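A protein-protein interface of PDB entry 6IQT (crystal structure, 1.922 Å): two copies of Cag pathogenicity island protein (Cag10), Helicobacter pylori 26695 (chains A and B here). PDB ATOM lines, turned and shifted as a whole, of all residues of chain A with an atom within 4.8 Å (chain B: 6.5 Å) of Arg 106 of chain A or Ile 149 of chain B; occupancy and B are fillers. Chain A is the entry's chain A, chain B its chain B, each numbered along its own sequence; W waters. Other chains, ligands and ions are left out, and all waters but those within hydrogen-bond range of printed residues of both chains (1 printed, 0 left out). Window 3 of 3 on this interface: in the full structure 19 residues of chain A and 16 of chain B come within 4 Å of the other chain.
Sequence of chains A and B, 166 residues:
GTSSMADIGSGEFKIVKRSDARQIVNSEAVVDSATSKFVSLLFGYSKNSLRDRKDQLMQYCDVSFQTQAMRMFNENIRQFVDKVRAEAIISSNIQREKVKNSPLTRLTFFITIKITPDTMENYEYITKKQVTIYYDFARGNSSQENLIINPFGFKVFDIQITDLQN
The guanidinium group of Arg 106 of chain A lies within salt-bridge range of the side-chain carboxylate of Asp 52 of chain B. The side-chain hydroxyl (OH) of Tyr 134 of chain A lies within hydrogen-bond range of the side-chain carboxylate (OD2) of Asp 52 of chain B. NE2 of Gln 56 of chain B lies within hydrogen-bond range of OH of Tyr 134 of chain A, 3.1 Å away.
N of Thr 108 of chain A sits at hydrogen-bond distance from O of Gln 95 of chain A, at 2.9 Å. The side-chain carboxylate (OE2) of Glu 97 of chain A lies within salt-bridge range of the guanidinium group (NH1) of Arg 106 of chain A. The backbone carbonyl oxygen (O) of Leu 104 of chain A is in hydrogen-bond range of the backbone NH (N) of Val 99 of chain A, at 3.0 Å. OE1 of Gln 56 of chain B is in hydrogen-bond range of NZ of Lys 37 of chain B (3.0 Å). OD2 of Asp 52 of chain B is in hydrogen-bond range of NE2 of Gln 56 of chain B, at 2.8 Å. The backbone carbonyl oxygen (O) of Ile 149 of chain B is in hydrogen-bond range of the side-chain hydroxyl (OH) of Tyr 60 of chain B (2.7 Å).
Among the printed residues, merely in contact across the chains: Arg 106 of chain A with Ile 149 of chain B, Thr 108 of chain A with Ile 148 of chain B, Gln 95 of chain A with Ile 148 of chain B, Arg 106 of chain A with Gln 56 of chain B, Val 99 of chain A with Asp 52 of chain B and Arg 96 of chain A with Ile 148 of chain B.
Of the printed residues of chain B, Gln 95 of chain A touches Ile 148. Printed residues of chain B within 4 Å of Arg 96 of chain A: Ile 148. Of the printed residues of chain B, Val 99 of chain A touches Asp 52. Thr 105 of chain A touches none of the printed residues of chain B. Of chain B, only Asp 52 (2.9 Å), Gln 56 (3.8 Å) and Ile 149 (3.3 Å) come within 4 Å of Arg 106 of chain A. Ile 133 of chain A touches none of the printed residues of chain B. Of the printed residues of chain B, Tyr 134 of chain A touches Asp 52 (2.5 Å) and Gln 56 (3.1 Å). Of the printed residues of chain A, Ile 148 of chain B touches Gln 95 (3.6 Å), Arg 96 (3.9 Å) and Thr 108 (3.5 Å). Of chain A, only Arg 106 (3.3 Å) comes within 4 Å of Ile 149 of chain B. The nearest residue of chain B that does not touch Arg 106 of chain A is Ile 148 of chain B (4.1 Å). The nearest residue of chain A that does not touch Ile 149 of chain B is Glu 97 of chain A (4.4 Å). The nearest printed residue of chain B that does not touch Tyr 134 of chain A is Leu 41 of chain B (6.4 Å).
Hydrophobic or aromatic side chains of chain B within 4 Å of the printed part of chain A: Ile 148 and Ile 149. Along chain B the printed residues that touch a printed residue of chain A span positions 52 to 149. Hydrophobic or aromatic side chains of chain A within 4 Å of the printed part of chain B: Val 99 and Tyr 134. Among the printed residues, 9 pairs touch across the chains. Among the printed residues, Asp or Glu carboxylates within 4 Å of a Lys or Arg side-chain nitrogen of the other chain: Arg 106 of chain A with Asp 52 of chain B (2.9 Å).
No position is printed for both chains.
Water W1 lies within hydrogen-bond range of NE2 of Gln 95 of chain A (2.9 Å) and O of Leu 147 of chain B (3.2 Å).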
ATOM      1  N   GLN A  95     -20.566  22.292   6.248  1.00  0.00           N
ATOM      2  CA  GLN A  95     -19.966  21.423   7.252  1.00  0.00           C
ATOM      3  C   GLN A  95     -19.458  20.143   6.603  1.00  0.00           C
ATOM      4  O   GLN A  95     -20.031  19.650   5.629  1.00  0.00           O
ATOM      5  CB  GLN A  95     -20.982  21.097   8.348  1.00  0.00           C
ATOM      6  CG  GLN A  95     -21.523  22.355   8.993  1.00  0.00           C
ATOM      7  CD  GLN A  95     -22.253  22.072  10.272  1.00  0.00           C
ATOM      8  OE1 GLN A  95     -21.658  22.064  11.350  1.00  0.00           O
ATOM      9  NE2 GLN A  95     -23.552  21.830  10.164  1.00  0.00           N
ATOM     10  N   ARG A  96     -18.365  19.609   7.144  1.00  0.00           N
ATOM     11  CA  ARG A  96     -17.701  18.495   6.489  1.00  0.00           C
ATOM     12  C   ARG A  96     -17.285  17.451   7.508  1.00  0.00           C
ATOM     13  O   ARG A  96     -16.951  17.767   8.653  1.00  0.00           O
ATOM     14  CB  ARG A  96     -16.473  18.947   5.680  1.00  0.00           C
ATOM     15  CG  ARG A  96     -15.401  19.694   6.466  1.00  0.00           C
ATOM     16  CD  ARG A  96     -14.612  20.560   5.503  1.00  0.00           C
ATOM     17  NE  ARG A  96     -15.310  21.816   5.263  1.00  0.00           N
ATOM     18  CZ  ARG A  96     -15.437  22.398   4.077  1.00  0.00           C
ATOM     19  NH1 ARG A  96     -14.921  21.840   2.992  1.00  0.00           N
ATOM     20  NH2 ARG A  96     -16.103  23.538   3.977  1.00  0.00           N
ATOM     21  N   GLU A  97     -17.295  16.197   7.068  1.00  0.00           N
ATOM     22  CA  GLU A  97     -16.904  15.095   7.931  1.00  0.00           C
ATOM     23  C   GLU A  97     -16.460  13.936   7.055  1.00  0.00           C
ATOM     24  O   GLU A  97     -17.160  13.575   6.101  1.00  0.00           O
ATOM     25  CB  GLU A  97     -18.076  14.683   8.833  1.00  0.00           C
ATOM     26  CG  GLU A  97     -17.703  13.822  10.022  1.00  0.00           C
ATOM     27  CD  GLU A  97     -18.702  13.940  11.183  1.00  0.00           C
ATOM     28  OE1 GLU A  97     -18.249  14.065  12.343  1.00  0.00           O
ATOM     29  OE2 GLU A  97     -19.932  13.906  10.945  1.00  0.00           O
ATOM     30  N   VAL A  99     -16.239  10.220   6.078  1.00  0.00           N
ATOM     31  CA  VAL A  99     -17.053   9.030   6.324  1.00  0.00           C
ATOM     32  C   VAL A  99     -16.133   7.925   6.834  1.00  0.00           C
ATOM     33  O   VAL A  99     -15.115   7.610   6.203  1.00  0.00           O
ATOM     34  CB  VAL A  99     -17.804   8.601   5.050  1.00  0.00           C
ATOM     35  CG1 VAL A  99     -18.552   7.279   5.266  1.00  0.00           C
ATOM     36  CG2 VAL A  99     -18.799   9.681   4.621  1.00  0.00           C
ATOM     37  N   LEU A 104     -14.660   8.485   1.144  1.00  0.00           N
ATOM     38  CA  LEU A 104     -15.548   9.611   0.855  1.00  0.00           C
ATOM     39  C   LEU A 104     -15.599  10.614   2.010  1.00  0.00           C
ATOM     40  O   LEU A 104     -15.372  10.276   3.175  1.00  0.00           O
ATOM     41  CB  LEU A 104     -16.968   9.114   0.552  1.00  0.00           C
ATOM     42  CG  LEU A 104     -17.135   8.111  -0.590  1.00  0.00           C
ATOM     43  CD1 LEU A 104     -18.557   7.576  -0.586  1.00  0.00           C
ATOM     44  CD2 LEU A 104     -16.808   8.788  -1.910  1.00  0.00           C
ATOM     45  N   THR A 105     -15.921  11.863   1.664  1.00  0.00           N
ATOM     46  CA  THR A 105     -16.171  12.931   2.620  1.00  0.00           C
ATOM     47  C   THR A 105     -17.602  13.421   2.425  1.00  0.00           C
ATOM     48  O   THR A 105     -18.067  13.561   1.288  1.00  0.00           O
ATOM     49  CB  THR A 105     -15.158  14.102   2.436  1.00  0.00           C
ATOM     50  OG1 THR A 105     -13.835  13.616   2.637  1.00  0.00           O
ATOM     51  CG2 THR A 105     -15.424  15.242   3.436  1.00  0.00           C
ATOM     52  N   ARG A 106     -18.298  13.662   3.536  1.00  0.00           N
ATOM     53  CA  ARG A 106     -19.678  14.145   3.538  1.00  0.00           C
ATOM     54  C   ARG A 106     -19.703  15.656   3.767  1.00  0.00           C
ATOM     55  O   ARG A 106     -19.118  16.147   4.730  1.00  0.00           O
ATOM     56  CB  ARG A 106     -20.484  13.446   4.640  1.00  0.00           C
ATOM     57  CG  ARG A 106     -21.992  13.725   4.593  1.00  0.00           C
ATOM     58  CD  ARG A 106     -22.577  13.874   5.993  1.00  0.00           C
ATOM     59  NE  ARG A 106     -22.256  12.755   6.869  1.00  0.00           N
ATOM     60  CZ  ARG A 106     -21.742  12.894   8.090  1.00  0.00           C
ATOM     61  NH1 ARG A 106     -21.474  14.105   8.565  1.00  0.00           N
ATOM     62  NH2 ARG A 106     -21.492  11.832   8.837  1.00  0.00           N
ATOM     63  N   LEU A 107     -20.381  16.384   2.884  1.00  0.00           N
ATOM     64  CA  LEU A 107     -20.625  17.810   3.043  1.00  0.00           C
ATOM     65  C   LEU A 107     -22.109  18.039   3.318  1.00  0.00           C
ATOM     66  O   LEU A 107     -22.964  17.395   2.707  1.00  0.00           O
ATOM     67  CB  LEU A 107     -20.196  18.568   1.778  1.00  0.00           C
ATOM     68  CG  LEU A 107     -18.754  18.428   1.272  1.00  0.00           C
ATOM     69  CD1 LEU A 107     -18.569  19.202  -0.040  1.00  0.00           C
ATOM     70  CD2 LEU A 107     -17.754  18.932   2.321  1.00  0.00           C
ATOM     71  N   THR A 108     -22.432  18.940   4.247  1.00  0.00           N
ATOM     72  CA  THR A 108     -23.838  19.239   4.523  1.00  0.00           C
ATOM     73  C   THR A 108     -24.039  20.753   4.540  1.00  0.00           C
ATOM     74  O   THR A 108     -23.222  21.494   5.097  1.00  0.00           O
ATOM     75  CB  THR A 108     -24.314  18.599   5.863  1.00  0.00           C
ATOM     76  OG1 THR A 108     -23.371  18.881   6.899  1.00  0.00           O
ATOM     77  CG2 THR A 108     -24.423  17.085   5.742  1.00  0.00           C
ATOM     78  N   THR A 132     -26.937  17.057   1.215  1.00  0.00           N
ATOM     79  CA  THR A 132     -25.759  16.299   1.619  1.00  0.00           C
ATOM     80  C   THR A 132     -25.090  15.741   0.370  1.00  0.00           C
ATOM     81  O   THR A 132     -25.742  15.069  -0.432  1.00  0.00           O
ATOM     82  CB  THR A 132     -26.162  15.132   2.530  1.00  0.00           C
ATOM     83  OG1 THR A 132     -26.908  15.620   3.649  1.00  0.00           O
ATOM     84  CG2 THR A 132     -24.944  14.360   2.997  1.00  0.00           C
ATOM     85  N   ILE A 133     -23.796  15.984   0.196  1.00  0.00           N
ATOM     86  CA  ILE A 133     -23.116  15.339  -0.922  1.00  0.00           C
ATOM     87  C   ILE A 133     -21.922  14.556  -0.391  1.00  0.00           C
ATOM     88  O   ILE A 133     -21.303  14.909   0.618  1.00  0.00           O
ATOM     89  CB  ILE A 133     -22.662  16.307  -2.049  1.00  0.00           C
ATOM     90  CG1 ILE A 133     -21.462  17.132  -1.622  1.00  0.00           C
ATOM     91  CG2 ILE A 133     -23.810  17.192  -2.601  1.00  0.00           C
ATOM     92  CD1 ILE A 133     -20.537  17.441  -2.777  1.00  0.00           C
ATOM     93  N   TYR A 134     -21.592  13.483  -1.098  1.00  0.00           N
ATOM     94  CA  TYR A 134     -20.424  12.669  -0.802  1.00  0.00           C
ATOM     95  C   TYR A 134     -19.463  12.796  -1.972  1.00  0.00           C
ATOM     96  O   TYR A 134     -19.873  12.635  -3.125  1.00  0.00           O
ATOM     97  CB  TYR A 134     -20.830  11.210  -0.583  1.00  0.00           C
ATOM     98  CG  TYR A 134     -21.782  11.011   0.579  1.00  0.00           C
ATOM     99  CD1 TYR A 134     -23.140  11.265   0.456  1.00  0.00           C
ATOM    100  CD2 TYR A 134     -21.313  10.574   1.806  1.00  0.00           C
ATOM    101  CE1 TYR A 134     -24.015  11.075   1.547  1.00  0.00           C
ATOM    102  CE2 TYR A 134     -22.159  10.403   2.880  1.00  0.00           C
ATOM    103  CZ  TYR A 134     -23.505  10.644   2.749  1.00  0.00           C
ATOM    104  OH  TYR A 134     -24.334  10.449   3.840  1.00  0.00           O
ATOM    105  N   LYS B  37     -35.896  13.689   7.975  1.00  0.00           N
ATOM    106  CA  LYS B  37     -34.546  13.129   7.871  1.00  0.00           C
ATOM    107  C   LYS B  37     -34.501  11.674   8.345  1.00  0.00           C
ATOM    108  O   LYS B  37     -33.926  10.811   7.671  1.00  0.00           O
ATOM    109  CB  LYS B  37     -33.564  13.990   8.674  1.00  0.00           C
ATOM    110  CG  LYS B  37     -32.102  13.590   8.445  1.00  0.00           C
ATOM    111  CD  LYS B  37     -31.670  13.859   7.027  1.00  0.00           C
ATOM    112  CE  LYS B  37     -30.214  13.477   6.838  1.00  0.00           C
ATOM    113  NZ  LYS B  37     -29.329  14.103   7.866  1.00  0.00           N
ATOM    114  N   LEU B  41     -33.577   8.399   6.077  1.00  0.00           N
ATOM    115  CA  LEU B  41     -32.495   7.489   6.418  1.00  0.00           C
ATOM    116  C   LEU B  41     -32.998   6.056   6.530  1.00  0.00           C
ATOM    117  O   LEU B  41     -32.402   5.137   5.966  1.00  0.00           O
ATOM    118  CB  LEU B  41     -31.850   7.924   7.729  1.00  0.00           C
ATOM    119  CG  LEU B  41     -31.047   9.226   7.702  1.00  0.00           C
ATOM    120  CD1 LEU B  41     -30.747   9.680   9.138  1.00  0.00           C
ATOM    121  CD2 LEU B  41     -29.759   9.060   6.884  1.00  0.00           C
ATOM    122  N   ASP B  52     -22.597   5.449   5.830  1.00  0.00           N
ATOM    123  CA  ASP B  52     -22.879   6.719   6.490  1.00  0.00           C
ATOM    124  C   ASP B  52     -24.369   6.882   6.775  1.00  0.00           C
ATOM    125  O   ASP B  52     -24.736   7.441   7.814  1.00  0.00           O
ATOM    126  CB  ASP B  52     -22.358   7.886   5.653  1.00  0.00           C
ATOM    127  CG  ASP B  52     -22.369   9.174   6.414  1.00  0.00           C
ATOM    128  OD1 ASP B  52     -21.638   9.282   7.434  1.00  0.00           O
ATOM    129  OD2 ASP B  52     -23.127  10.085   6.027  1.00  0.00           O
ATOM    130  N   ASP B  55     -24.786   5.105   9.959  1.00  0.00           N
ATOM    131  CA  ASP B  55     -24.241   5.942  11.030  1.00  0.00           C
ATOM    132  C   ASP B  55     -25.199   7.063  11.405  1.00  0.00           C
ATOM    133  O   ASP B  55     -25.449   7.312  12.591  1.00  0.00           O
ATOM    134  CB  ASP B  55     -22.901   6.547  10.599  1.00  0.00           C
ATOM    135  CG  ASP B  55     -21.756   5.559  10.683  1.00  0.00           C
ATOM    136  OD1 ASP B  55     -21.986   4.415  11.136  1.00  0.00           O
ATOM    137  OD2 ASP B  55     -20.628   5.919  10.277  1.00  0.00           O
ATOM    138  N   GLN B  56     -25.718   7.782  10.405  1.00  0.00           N
ATOM    139  CA  GLN B  56     -26.623   8.888  10.705  1.00  0.00           C
ATOM    140  C   GLN B  56     -27.887   8.395  11.403  1.00  0.00           C
ATOM    141  O   GLN B  56     -28.365   9.023  12.358  1.00  0.00           O
ATOM    142  CB  GLN B  56     -26.983   9.626   9.423  1.00  0.00           C
ATOM    143  CG  GLN B  56     -25.799  10.304   8.731  1.00  0.00           C
ATOM    144  CD  GLN B  56     -26.285  11.251   7.678  1.00  0.00           C
ATOM    145  OE1 GLN B  56     -27.233  11.990   7.909  1.00  0.00           O
ATOM    146  NE2 GLN B  56     -25.671  11.218   6.512  1.00  0.00           N
ATOM    147  N   LEU B  57     -28.458   7.283  10.921  1.00  0.00           N
ATOM    148  CA  LEU B  57     -29.693   6.770  11.509  1.00  0.00           C
ATOM    149  C   LEU B  57     -29.545   6.532  13.010  1.00  0.00           C
ATOM    150  O   LEU B  57     -30.449   6.857  13.787  1.00  0.00           O
ATOM    151  CB  LEU B  57     -30.114   5.474  10.808  1.00  0.00           C
ATOM    152  CG  LEU B  57     -31.387   4.816  11.335  1.00  0.00           C
ATOM    153  CD1 LEU B  57     -32.621   5.724  11.106  1.00  0.00           C
ATOM    154  CD2 LEU B  57     -31.565   3.490  10.647  1.00  0.00           C
ATOM    155  N   GLN B  59     -27.703   8.136  15.114  1.00  0.00           N
ATOM    156  CA  GLN B  59     -27.704   9.408  15.835  1.00  0.00           C
ATOM    157  C   GLN B  59     -29.106   9.953  16.066  1.00  0.00           C
ATOM    158  O   GLN B  59     -29.292  10.783  16.962  1.00  0.00           O
ATOM    159  CB  GLN B  59     -26.890  10.456  15.083  1.00  0.00           C
ATOM    160  CG  GLN B  59     -25.415  10.189  15.089  1.00  0.00           C
ATOM    161  CD  GLN B  59     -24.843  10.188  16.487  1.00  0.00           C
ATOM    162  OE1 GLN B  59     -25.030  11.142  17.254  1.00  0.00           O
ATOM    163  NE2 GLN B  59     -24.146   9.109  16.836  1.00  0.00           N
ATOM    164  N   TYR B  60     -30.085   9.525  15.269  1.00  0.00           N
ATOM    165  CA  TYR B  60     -31.480   9.916  15.440  1.00  0.00           C
ATOM    166  C   TYR B  60     -32.278   8.958  16.326  1.00  0.00           C
ATOM    167  O   TYR B  60     -33.490   9.151  16.482  1.00  0.00           O
ATOM    168  CB  TYR B  60     -32.145  10.036  14.061  1.00  0.00           C
ATOM    169  CG  TYR B  60     -31.820  11.349  13.394  1.00  0.00           C
ATOM    170  CD1 TYR B  60     -30.702  11.493  12.577  1.00  0.00           C
ATOM    171  CD2 TYR B  60     -32.619  12.464  13.610  1.00  0.00           C
ATOM    172  CE1 TYR B  60     -30.415  12.722  11.981  1.00  0.00           C
ATOM    173  CE2 TYR B  60     -32.331  13.683  13.033  1.00  0.00           C
ATOM    174  CZ  TYR B  60     -31.240  13.815  12.226  1.00  0.00           C
ATOM    175  OH  TYR B  60     -31.002  15.057  11.673  1.00  0.00           O
ATOM    176  N   LEU B 147     -23.700  16.306  16.127  1.00  0.00           N
ATOM    177  CA  LEU B 147     -24.248  17.665  16.081  1.00  0.00           C
ATOM    178  C   LEU B 147     -24.250  18.254  14.657  1.00  0.00           C
ATOM    179  O   LEU B 147     -25.107  19.080  14.309  1.00  0.00           O
ATOM    180  CB  LEU B 147     -23.478  18.574  17.030  1.00  0.00           C
ATOM    181  CG  LEU B 147     -24.304  19.705  17.650  1.00  0.00           C
ATOM    182  CD1 LEU B 147     -23.669  20.158  18.947  1.00  0.00           C
ATOM    183  CD2 LEU B 147     -24.440  20.879  16.688  1.00  0.00           C
ATOM    184  N   ILE B 148     -23.305  17.826  13.820  1.00  0.00           N
ATOM    185  CA  ILE B 148     -23.447  18.093  12.390  1.00  0.00           C
ATOM    186  C   ILE B 148     -24.673  17.370  11.854  1.00  0.00           C
ATOM    187  O   ILE B 148     -25.464  17.929  11.087  1.00  0.00           O
ATOM    188  CB  ILE B 148     -22.174  17.676  11.632  1.00  0.00           C
ATOM    189  CG1 ILE B 148     -20.994  18.564  12.038  1.00  0.00           C
ATOM    190  CG2 ILE B 148     -22.404  17.748  10.120  1.00  0.00           C
ATOM    191  CD1 ILE B 148     -19.670  18.115  11.432  1.00  0.00           C
ATOM    192  N   ILE B 149     -24.873  16.128  12.290  1.00  0.00           N
ATOM    193  CA  ILE B 149     -25.903  15.258  11.727  1.00  0.00           C
ATOM    194  C   ILE B 149     -27.268  15.523  12.355  1.00  0.00           C
ATOM    195  O   ILE B 149     -28.306  15.450  11.679  1.00  0.00           O
ATOM    196  CB  ILE B 149     -25.456  13.794  11.909  1.00  0.00           C
ATOM    197  CG1 ILE B 149     -24.293  13.503  10.959  1.00  0.00           C
ATOM    198  CG2 ILE B 149     -26.626  12.805  11.776  1.00  0.00           C
ATOM    199  CD1 ILE B 149     -24.621  13.836   9.500  1.00  0.00           C
ATOM    200  N   ASN B 150     -27.298  15.829  13.648  1.00  0.00           N
ATOM    201  CA  ASN B 150     -28.553  15.950  14.399  1.00  0.00           C
ATOM    202  C   ASN B 150     -28.402  17.130  15.357  1.00  0.00           C
ATOM    203  O   ASN B 150     -28.244  16.958  16.569  1.00  0.00           O
ATOM    204  CB  ASN B 150     -28.859  14.639  15.133  1.00  0.00           C
ATOM    205  CG  ASN B 150     -30.199  14.654  15.879  1.00  0.00           C
ATOM    206  OD1 ASN B 150     -31.027  15.560  15.718  1.00  0.00           O
ATOM    207  ND2 ASN B 150     -30.415  13.625  16.686  1.00  0.00           N
ATOM    208  N   PRO B 151     -28.431  18.357  14.825  1.00  0.00           N
ATOM    209  CA  PRO B 151     -28.051  19.523  15.647  1.00  0.00           C
ATOM    210  C   PRO B 151     -29.003  19.822  16.794  1.00  0.00           C
ATOM    211  O   PRO B 151     -28.587  20.487  17.748  1.00  0.00           O
ATOM    212  CB  PRO B 151     -28.025  20.674  14.629  1.00  0.00           C
ATOM    213  CG  PRO B 151     -28.919  20.216  13.510  1.00  0.00           C
ATOM    214  CD  PRO B 151     -28.707  18.724  13.425  1.00  0.00           C
HETATM  215  O   HOH W   1     -25.036  21.885  12.678  1.00  0.00           O
